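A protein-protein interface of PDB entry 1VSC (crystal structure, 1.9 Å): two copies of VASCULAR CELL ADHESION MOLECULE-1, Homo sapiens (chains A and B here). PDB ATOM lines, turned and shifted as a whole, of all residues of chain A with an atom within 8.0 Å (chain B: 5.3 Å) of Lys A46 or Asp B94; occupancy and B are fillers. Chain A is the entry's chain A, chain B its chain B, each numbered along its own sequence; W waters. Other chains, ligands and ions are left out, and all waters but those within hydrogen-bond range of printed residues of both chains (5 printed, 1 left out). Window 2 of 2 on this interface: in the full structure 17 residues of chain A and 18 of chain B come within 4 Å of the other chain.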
ATOM      1  N   VAL A  19     -18.111 -28.115  36.356  1.00  0.00           N
ATOM      2  CA  VAL A  19     -18.485 -29.499  36.115  1.00  0.00           C
ATOM      3  C   VAL A  19     -17.451 -30.248  35.250  1.00  0.00           C
ATOM      4  O   VAL A  19     -17.017 -29.722  34.223  1.00  0.00           O
ATOM      5  CB  VAL A  19     -19.819 -29.470  35.377  1.00  0.00           C
ATOM      6  CG1 VAL A  19     -20.243 -30.839  34.944  1.00  0.00           C
ATOM      7  CG2 VAL A  19     -20.864 -28.816  36.252  1.00  0.00           C
ATOM      8  N   SER A  20     -17.130 -31.485  35.625  1.00  0.00           N
ATOM      9  CA  SER A  20     -16.170 -32.311  34.892  1.00  0.00           C
ATOM     10  C   SER A  20     -16.718 -33.644  34.381  1.00  0.00           C
ATOM     11  O   SER A  20     -17.373 -34.385  35.114  1.00  0.00           O
ATOM     12  CB  SER A  20     -14.981 -32.619  35.772  1.00  0.00           C
ATOM     13  OG  SER A  20     -14.076 -31.552  35.702  1.00  0.00           O
ATOM     14  N   LEU A  21     -16.472 -33.925  33.106  1.00  0.00           N
ATOM     15  CA  LEU A  21     -16.889 -35.202  32.499  1.00  0.00           C
ATOM     16  C   LEU A  21     -15.597 -35.900  32.083  1.00  0.00           C
ATOM     17  O   LEU A  21     -14.749 -35.282  31.454  1.00  0.00           O
ATOM     18  CB  LEU A  21     -17.704 -34.968  31.239  1.00  0.00           C
ATOM     19  CG  LEU A  21     -18.898 -34.039  31.275  1.00  0.00           C
ATOM     20  CD1 LEU A  21     -19.642 -34.267  29.975  1.00  0.00           C
ATOM     21  CD2 LEU A  21     -19.808 -34.332  32.488  1.00  0.00           C
ATOM     22  N   TRP A  35     -14.349 -34.944  21.993  1.00  0.00           N
ATOM     23  CA  TRP A  35     -15.699 -34.763  22.474  1.00  0.00           C
ATOM     24  C   TRP A  35     -16.383 -33.890  21.506  1.00  0.00           C
ATOM     25  O   TRP A  35     -15.741 -33.120  20.798  1.00  0.00           O
ATOM     26  CB  TRP A  35     -15.684 -34.057  23.817  1.00  0.00           C
ATOM     27  CG  TRP A  35     -15.065 -34.820  24.943  1.00  0.00           C
ATOM     28  CD1 TRP A  35     -13.759 -34.874  25.272  1.00  0.00           C
ATOM     29  CD2 TRP A  35     -15.761 -35.504  25.965  1.00  0.00           C
ATOM     30  NE1 TRP A  35     -13.587 -35.539  26.462  1.00  0.00           N
ATOM     31  CE2 TRP A  35     -14.817 -35.928  26.909  1.00  0.00           C
ATOM     32  CE3 TRP A  35     -17.099 -35.777  26.187  1.00  0.00           C
ATOM     33  CZ2 TRP A  35     -15.170 -36.618  28.063  1.00  0.00           C
ATOM     34  CZ3 TRP A  35     -17.458 -36.473  27.345  1.00  0.00           C
ATOM     35  CH2 TRP A  35     -16.505 -36.876  28.258  1.00  0.00           C
ATOM     36  N   LEU A  43     -17.835 -26.839  22.335  1.00  0.00           N
ATOM     37  CA  LEU A  43     -17.891 -27.562  23.583  1.00  0.00           C
ATOM     38  C   LEU A  43     -18.143 -26.588  24.728  1.00  0.00           C
ATOM     39  O   LEU A  43     -18.843 -26.937  25.705  1.00  0.00           O
ATOM     40  CB  LEU A  43     -16.613 -28.356  23.834  1.00  0.00           C
ATOM     41  CG  LEU A  43     -16.370 -29.642  23.010  1.00  0.00           C
ATOM     42  CD1 LEU A  43     -15.405 -30.417  23.806  1.00  0.00           C
ATOM     43  CD2 LEU A  43     -17.577 -30.516  22.792  1.00  0.00           C
ATOM     44  N   ASN A  44     -17.598 -25.375  24.617  1.00  0.00           N
ATOM     45  CA  ASN A  44     -17.803 -24.370  25.670  1.00  0.00           C
ATOM     46  C   ASN A  44     -17.273 -24.989  26.964  1.00  0.00           C
ATOM     47  O   ASN A  44     -17.894 -24.942  28.012  1.00  0.00           O
ATOM     48  CB  ASN A  44     -19.289 -23.998  25.741  1.00  0.00           C
ATOM     49  CG  ASN A  44     -19.762 -23.292  24.497  1.00  0.00           C
ATOM     50  OD1 ASN A  44     -19.003 -22.610  23.863  1.00  0.00           O
ATOM     51  ND2 ASN A  44     -21.004 -23.488  24.108  1.00  0.00           N
ATOM     52  N   GLY A  45     -16.098 -25.596  26.849  1.00  0.00           N
ATOM     53  CA  GLY A  45     -15.450 -26.226  27.982  1.00  0.00           C
ATOM     54  C   GLY A  45     -14.047 -26.577  27.520  1.00  0.00           C
ATOM     55  O   GLY A  45     -13.750 -26.469  26.318  1.00  0.00           O
ATOM     56  N   LYS A  46     -13.208 -27.054  28.436  1.00  0.00           N
ATOM     57  CA  LYS A  46     -11.829 -27.379  28.105  1.00  0.00           C
ATOM     58  C   LYS A  46     -11.462 -28.846  28.225  1.00  0.00           C
ATOM     59  O   LYS A  46     -11.450 -29.395  29.341  1.00  0.00           O
ATOM     60  CB  LYS A  46     -10.858 -26.622  29.003  1.00  0.00           C
ATOM     61  CG  LYS A  46      -9.393 -26.923  28.694  1.00  0.00           C
ATOM     62  CD  LYS A  46      -8.474 -26.208  29.675  1.00  0.00           C
ATOM     63  CE  LYS A  46      -7.637 -25.135  28.965  1.00  0.00           C
ATOM     64  NZ  LYS A  46      -8.403 -24.289  27.959  1.00  0.00           N
ATOM     65  N   VAL A  47     -11.000 -29.421  27.111  1.00  0.00           N
ATOM     66  CA  VAL A  47     -10.575 -30.836  27.070  1.00  0.00           C
ATOM     67  C   VAL A  47      -9.100 -31.056  27.401  1.00  0.00           C
ATOM     68  O   VAL A  47      -8.234 -30.370  26.867  1.00  0.00           O
ATOM     69  CB  VAL A  47     -10.826 -31.455  25.688  1.00  0.00           C
ATOM     70  CG1 VAL A  47     -10.552 -32.993  25.740  1.00  0.00           C
ATOM     71  CG2 VAL A  47     -12.245 -31.118  25.221  1.00  0.00           C
ATOM     72  N   THR A  48      -8.825 -31.980  28.316  1.00  0.00           N
ATOM     73  CA  THR A  48      -7.460 -32.348  28.677  1.00  0.00           C
ATOM     74  C   THR A  48      -7.330 -33.879  28.677  1.00  0.00           C
ATOM     75  O   THR A  48      -8.104 -34.596  29.298  1.00  0.00           O
ATOM     76  CB  THR A  48      -7.073 -31.794  30.027  1.00  0.00           C
ATOM     77  OG1 THR A  48      -8.035 -32.225  30.993  1.00  0.00           O
ATOM     78  CG2 THR A  48      -7.034 -30.245  29.977  1.00  0.00           C
ATOM     79  N   ASN A  49      -6.328 -34.359  27.962  1.00  0.00           N
ATOM     80  CA  ASN A  49      -6.073 -35.778  27.812  1.00  0.00           C
ATOM     81  C   ASN A  49      -4.849 -36.187  28.582  1.00  0.00           C
ATOM     82  O   ASN A  49      -3.796 -35.609  28.404  1.00  0.00           O
ATOM     83  CB  ASN A  49      -5.910 -36.091  26.320  1.00  0.00           C
ATOM     84  CG  ASN A  49      -7.223 -35.899  25.540  1.00  0.00           C
ATOM     85  OD1 ASN A  49      -8.264 -35.592  26.136  1.00  0.00           O
ATOM     86  ND2 ASN A  49      -7.194 -36.108  24.222  1.00  0.00           N
ATOM     87  N   SER A  54      -9.835 -38.793  29.176  1.00  0.00           N
ATOM     88  CA  SER A  54      -9.972 -37.418  28.676  1.00  0.00           C
ATOM     89  C   SER A  54     -10.937 -36.687  29.656  1.00  0.00           C
ATOM     90  O   SER A  54     -11.836 -37.315  30.235  1.00  0.00           O
ATOM     91  CB  SER A  54     -10.577 -37.425  27.281  1.00  0.00           C
ATOM     92  OG  SER A  54     -10.809 -36.111  26.781  1.00  0.00           O
ATOM     93  N   THR A  55     -10.681 -35.418  29.963  1.00  0.00           N
ATOM     94  CA  THR A  55     -11.605 -34.690  30.834  1.00  0.00           C
ATOM     95  C   THR A  55     -12.150 -33.438  30.111  1.00  0.00           C
ATOM     96  O   THR A  55     -11.403 -32.715  29.417  1.00  0.00           O
ATOM     97  CB  THR A  55     -10.956 -34.257  32.156  1.00  0.00           C
ATOM     98  OG1 THR A  55     -10.230 -35.338  32.718  1.00  0.00           O
ATOM     99  CG2 THR A  55     -12.007 -33.919  33.159  1.00  0.00           C
ATOM    100  N   LEU A  56     -13.467 -33.274  30.133  1.00  0.00           N
ATOM    101  CA  LEU A  56     -14.078 -32.087  29.576  1.00  0.00           C
ATOM    102  C   LEU A  56     -14.523 -31.312  30.809  1.00  0.00           C
ATOM    103  O   LEU A  56     -15.397 -31.760  31.528  1.00  0.00           O
ATOM    104  CB  LEU A  56     -15.285 -32.380  28.702  1.00  0.00           C
ATOM    105  CG  LEU A  56     -16.089 -31.166  28.190  1.00  0.00           C
ATOM    106  CD1 LEU A  56     -15.282 -30.233  27.307  1.00  0.00           C
ATOM    107  CD2 LEU A  56     -17.248 -31.700  27.394  1.00  0.00           C
ATOM    108  N   THR A  57     -13.807 -30.226  31.086  1.00  0.00           N
ATOM    109  CA  THR A  57     -14.051 -29.316  32.221  1.00  0.00           C
ATOM    110  C   THR A  57     -14.900 -28.100  31.813  1.00  0.00           C
ATOM    111  O   THR A  57     -14.545 -27.366  30.890  1.00  0.00           O
ATOM    112  CB  THR A  57     -12.714 -28.841  32.792  1.00  0.00           C
ATOM    113  OG1 THR A  57     -11.984 -29.989  33.226  1.00  0.00           O
ATOM    114  CG2 THR A  57     -12.925 -27.874  33.992  1.00  0.00           C
ATOM    115  N   MET A  58     -16.066 -27.946  32.434  1.00  0.00           N
ATOM    116  CA  MET A  58     -16.936 -26.812  32.126  1.00  0.00           C
ATOM    117  C   MET A  58     -17.074 -25.987  33.420  1.00  0.00           C
ATOM    118  O   MET A  58     -17.729 -26.356  34.378  1.00  0.00           O
ATOM    119  CB  MET A  58     -18.283 -27.257  31.578  1.00  0.00           C
ATOM    120  CG  MET A  58     -18.191 -27.972  30.257  1.00  0.00           C
ATOM    121  SD  MET A  58     -19.611 -29.113  30.065  1.00  0.00           S
ATOM    122  CE  MET A  58     -19.402 -30.152  31.553  1.00  0.00           C
ATOM    123  N   ASN A  59     -16.331 -24.903  33.435  1.00  0.00           N
ATOM    124  CA  ASN A  59     -16.263 -24.077  34.577  1.00  0.00           C
ATOM    125  C   ASN A  59     -16.146 -22.618  34.105  1.00  0.00           C
ATOM    126  O   ASN A  59     -15.100 -22.174  33.635  1.00  0.00           O
ATOM    127  CB  ASN A  59     -15.062 -24.525  35.384  1.00  0.00           C
ATOM    128  CG  ASN A  59     -14.857 -23.691  36.612  1.00  0.00           C
ATOM    129  OD1 ASN A  59     -15.819 -23.288  37.247  1.00  0.00           O
ATOM    130  ND2 ASN A  59     -13.602 -23.390  36.932  1.00  0.00           N
ATOM    131  N   ASN A  65     -23.623 -25.179  27.676  1.00  0.00           N
ATOM    132  CA  ASN A  65     -23.259 -26.487  28.123  1.00  0.00           C
ATOM    133  C   ASN A  65     -24.487 -27.358  28.272  1.00  0.00           C
ATOM    134  O   ASN A  65     -24.390 -28.476  28.771  1.00  0.00           O
ATOM    135  CB  ASN A  65     -22.511 -26.391  29.432  1.00  0.00           C
ATOM    136  CG  ASN A  65     -21.194 -25.662  29.298  1.00  0.00           C
ATOM    137  OD1 ASN A  65     -20.917 -24.696  30.029  1.00  0.00           O
ATOM    138  ND2 ASN A  65     -20.333 -26.144  28.384  1.00  0.00           N
ATOM    139  N   PRO B  92     -14.347 -16.003  31.088  1.00  0.00           N
ATOM    140  CA  PRO B  92     -13.808 -17.185  31.787  1.00  0.00           C
ATOM    141  C   PRO B  92     -13.181 -18.381  31.022  1.00  0.00           C
ATOM    142  O   PRO B  92     -12.592 -19.263  31.625  1.00  0.00           O
ATOM    143  CB  PRO B  92     -15.048 -17.682  32.528  1.00  0.00           C
ATOM    144  CG  PRO B  92     -16.117 -17.530  31.442  1.00  0.00           C
ATOM    145  CD  PRO B  92     -15.817 -16.110  30.919  1.00  0.00           C
ATOM    146  N   LYS B  93     -13.394 -18.454  29.717  1.00  0.00           N
ATOM    147  CA  LYS B  93     -12.932 -19.606  28.922  1.00  0.00           C
ATOM    148  C   LYS B  93     -12.132 -19.208  27.685  1.00  0.00           C
ATOM    149  O   LYS B  93     -12.460 -18.224  27.011  1.00  0.00           O
ATOM    150  CB  LYS B  93     -14.163 -20.419  28.475  1.00  0.00           C
ATOM    151  CG  LYS B  93     -14.904 -21.133  29.619  1.00  0.00           C
ATOM    152  CD  LYS B  93     -16.294 -21.517  29.196  1.00  0.00           C
ATOM    153  CE  LYS B  93     -16.964 -22.409  30.269  1.00  0.00           C
ATOM    154  NZ  LYS B  93     -18.419 -22.565  29.906  1.00  0.00           N
ATOM    155  N   ASP B  94     -11.101 -20.004  27.386  1.00  0.00           N
ATOM    156  CA  ASP B  94     -10.290 -19.772  26.201  1.00  0.00           C
ATOM    157  C   ASP B  94     -11.158 -20.072  24.998  1.00  0.00           C
ATOM    158  O   ASP B  94     -12.186 -20.768  25.089  1.00  0.00           O
ATOM    159  CB  ASP B  94      -9.100 -20.699  26.190  1.00  0.00           C
ATOM    160  CG  ASP B  94      -8.114 -20.383  27.262  1.00  0.00           C
ATOM    161  OD1 ASP B  94      -7.933 -19.189  27.568  1.00  0.00           O
ATOM    162  OD2 ASP B  94      -7.498 -21.342  27.794  1.00  0.00           O
ATOM    163  N   PRO B  95     -10.833 -19.472  23.866  1.00  0.00           N
ATOM    164  CA  PRO B  95     -11.649 -19.753  22.691  1.00  0.00           C
ATOM    165  C   PRO B  95     -11.388 -21.222  22.254  1.00  0.00           C
ATOM    166  O   PRO B  95     -10.475 -21.880  22.784  1.00  0.00           O
ATOM    167  CB  PRO B  95     -11.096 -18.757  21.674  1.00  0.00           C
ATOM    168  CG  PRO B  95      -9.706 -18.623  22.078  1.00  0.00           C
ATOM    169  CD  PRO B  95      -9.752 -18.538  23.555  1.00  0.00           C
ATOM    170  N   GLU B  96     -12.145 -21.702  21.271  1.00  0.00           N
ATOM    171  CA  GLU B  96     -12.015 -23.101  20.789  1.00  0.00           C
ATOM    172  C   GLU B  96     -11.995 -23.144  19.276  1.00  0.00           C
ATOM    173  O   GLU B  96     -12.900 -22.577  18.627  1.00  0.00           O
ATOM    174  CB  GLU B  96     -13.238 -23.927  21.207  1.00  0.00           C
ATOM    175  CG  GLU B  96     -13.227 -24.380  22.651  1.00  0.00           C
ATOM    176  CD  GLU B  96     -14.646 -24.562  23.244  1.00  0.00           C
ATOM    177  OE1 GLU B  96     -15.594 -24.733  22.472  1.00  0.00           O
ATOM    178  OE2 GLU B  96     -14.817 -24.471  24.492  1.00  0.00           O
ATOM    179  N   SER B 114     -14.472 -19.969  18.232  1.00  0.00           N
ATOM    180  CA  SER B 114     -15.513 -19.437  19.111  1.00  0.00           C
ATOM    181  C   SER B 114     -15.116 -19.211  20.558  1.00  0.00           C
ATOM    182  O   SER B 114     -14.150 -19.795  21.052  1.00  0.00           O
ATOM    183  CB  SER B 114     -16.685 -20.406  19.088  1.00  0.00           C
ATOM    184  OG  SER B 114     -16.277 -21.640  19.664  1.00  0.00           O
ATOM    185  N   VAL B 115     -15.875 -18.369  21.274  1.00  0.00           N
ATOM    186  CA  VAL B 115     -15.570 -18.129  22.710  1.00  0.00           C
ATOM    187  C   VAL B 115     -16.880 -18.162  23.423  1.00  0.00           C
ATOM    188  O   VAL B 115     -17.884 -17.629  22.922  1.00  0.00           O
ATOM    189  CB  VAL B 115     -14.987 -16.762  23.078  1.00  0.00           C
ATOM    190  CG1 VAL B 115     -13.912 -16.964  24.098  1.00  0.00           C
ATOM    191  CG2 VAL B 115     -14.528 -16.001  21.870  1.00  0.00           C
ATOM    192  N   ALA B 116     -16.858 -18.824  24.572  1.00  0.00           N
ATOM    193  CA  ALA B 116     -18.044 -18.983  25.418  1.00  0.00           C
ATOM    194  C   ALA B 116     -18.140 -17.979  26.583  1.00  0.00           C
ATOM    195  O   ALA B 116     -17.121 -17.617  27.169  1.00  0.00           O
ATOM    196  CB  ALA B 116     -18.043 -20.396  26.011  1.00  0.00           C
ATOM    197  N   ARG B 187      -7.301 -14.367  25.463  1.00  0.00           N
ATOM    198  CA  ARG B 187      -7.279 -15.792  25.755  1.00  0.00           C
ATOM    199  C   ARG B 187      -7.162 -16.349  24.335  1.00  0.00           C
ATOM    200  O   ARG B 187      -7.831 -15.868  23.422  1.00  0.00           O
ATOM    201  CB  ARG B 187      -8.609 -16.259  26.381  1.00  0.00           C
ATOM    202  CG  ARG B 187      -8.818 -15.979  27.876  1.00  0.00           C
ATOM    203  CD  ARG B 187      -9.949 -16.843  28.441  1.00  0.00           C
ATOM    204  NE  ARG B 187     -10.137 -16.675  29.884  1.00  0.00           N
ATOM    205  CZ  ARG B 187      -9.724 -17.531  30.821  1.00  0.00           C
ATOM    206  NH1 ARG B 187      -9.085 -18.653  30.505  1.00  0.00           N
ATOM    207  NH2 ARG B 187      -9.926 -17.239  32.104  1.00  0.00           N
ATOM    208  N   GLN B 188      -6.317 -17.340  24.120  1.00  0.00           N
ATOM    209  CA  GLN B 188      -6.215 -17.863  22.767  1.00  0.00           C
ATOM    210  C   GLN B 188      -6.142 -19.370  22.698  1.00  0.00           C
ATOM    211  O   GLN B 188      -5.930 -20.067  23.682  1.00  0.00           O
ATOM    212  CB  GLN B 188      -5.040 -17.281  22.042  1.00  0.00           C
ATOM    213  CG  GLN B 188      -3.756 -17.704  22.657  1.00  0.00           C
ATOM    214  CD  GLN B 188      -2.593 -17.444  21.733  1.00  0.00           C
ATOM    215  OE1 GLN B 188      -2.305 -16.295  21.361  1.00  0.00           O
ATOM    216  NE2 GLN B 188      -1.920 -18.519  21.337  1.00  0.00           N
HETATM  217  O   HOH W   1     -12.677 -21.596  32.811  1.00  0.00           O
HETATM  218  O   HOH W   2     -16.701 -22.055  22.526  1.00  0.00           O
HETATM  219  O   HOH W   3     -10.804 -22.505  28.862  1.00  0.00           O
HETATM  220  O   HOH W   4     -15.549 -26.722  20.847  1.00  0.00           O
HETATM  221  O   HOH W   5     -21.114 -22.172  28.311  1.00  0.00           O
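The backbone NH (N) of Leu A43 lies within hydrogen-bond range of the side-chain carboxylate (OE1) of Glu B96 (3.1 Å). The backbone NH of Gly A45 lies within hydrogen-bond range of the side-chain carboxylate of Glu B96 (2.9 Å). The backbone NH (N) of Asn A44 lies within hydrogen-bond range of the side-chain carboxylate (OE2) of Glu B96 (2.9 Å). The side-chain amino group (NZ) of Lys B93 is in hydrogen-bond range of the side-chain amide oxygen (OD1) of Asn A65. The side-chain carboxylate (OD2) of Asp B94 lies within salt-bridge range of the side-chain amino group (NZ) of Lys A46, at 3.1 Å. The backbone carbonyl oxygen (O) of Asn A44 sits at hydrogen-bond distance from the side-chain amino group (NZ) of Lys B93 (3.1 Å).
The side-chain sulfur of Met A58 sits close to the side-chain amide nitrogen of Asn A65 (3.5 Å). N of Glu B96 sits at hydrogen-bond distance from O of Ser B114. ND2 of Asn A65 lies within hydrogen-bond range of O of Asn A44 (2.7 Å). The side-chain amide nitrogen (ND2) of Asn A65 is in hydrogen-bond range of the backbone carbonyl oxygen (O) of Leu A43 (3.2 Å). NH1 of Arg B187 lies within salt-bridge range of OD1 of Asp B94 (3.2 Å). The backbone carbonyl oxygen (O) of Thr A57 lies within hydrogen-bond range of the backbone NH (N) of Lys A46 (2.8 Å).
Among the printed residues, merely in contact across the chains: Asn A44 with Ala B116 and Asn A59 with Lys B93.
Of chain B, only Asp B94 comes within 4 Å of Lys A46. Of chain A, only Lys A46 (3.1 Å) comes within 4 Å of Asp B94. Pro B95 touches none of the printed residues of chain A. Of the printed residues of chain B, Asn A44 touches Lys B93, Glu B96 and Ala B116. Printed residues of chain B within 4 Å of Asn A65: Lys B93 (3.3 Å). Of the printed residues of chain A, Glu B96 touches Leu A43 (3.1 Å), Asn A44 (2.9 Å) and Gly A45 (2.9 Å). Printed residues of chain A within 4 Å of Lys B93: Asn A44, Asn A59 and Asn A65. Of the printed residues of chain B, Leu A43 touches Glu B96 (3.1 Å). Leu A56 touches none of the printed residues of chain B. The nearest printed residue of chain A that does not touch Ala B116 is Gly A45 (5.6 Å).
Printed residues of chain A that touch a printed residue of chain B: Leu A43, Asn A44, Gly A45, Lys A46, Asn A59 and Asn A65. Among the printed residues, 8 pairs touch across the chains.
No position is printed for both chains.
Water W4 bridges the side-chain carboxylate (OE1) of Glu B96 and the backbone NH (N) of Leu A43. Water W1 lies within hydrogen-bond range of O of Pro B92 and O of Asn A59. Water W2 lies within hydrogen-bond range of the side-chain amide oxygen (OD1) of Asn A44 (2.7 Å), the side-chain carboxylate (OE1) of Glu B96 (2.9 Å) and the side-chain hydroxyl (OG) of Ser B114 (2.9 Å). Water W3 lies within hydrogen-bond range of the backbone NH (N) of Asp B94 (2.9 Å) and the side-chain amino group (NZ) of Lys A46 (3.1 Å). Water W5 lies within hydrogen-bond range of OD1 of Asn A65 (3.1 Å) and NZ of Lys B93 (3.2 Å).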
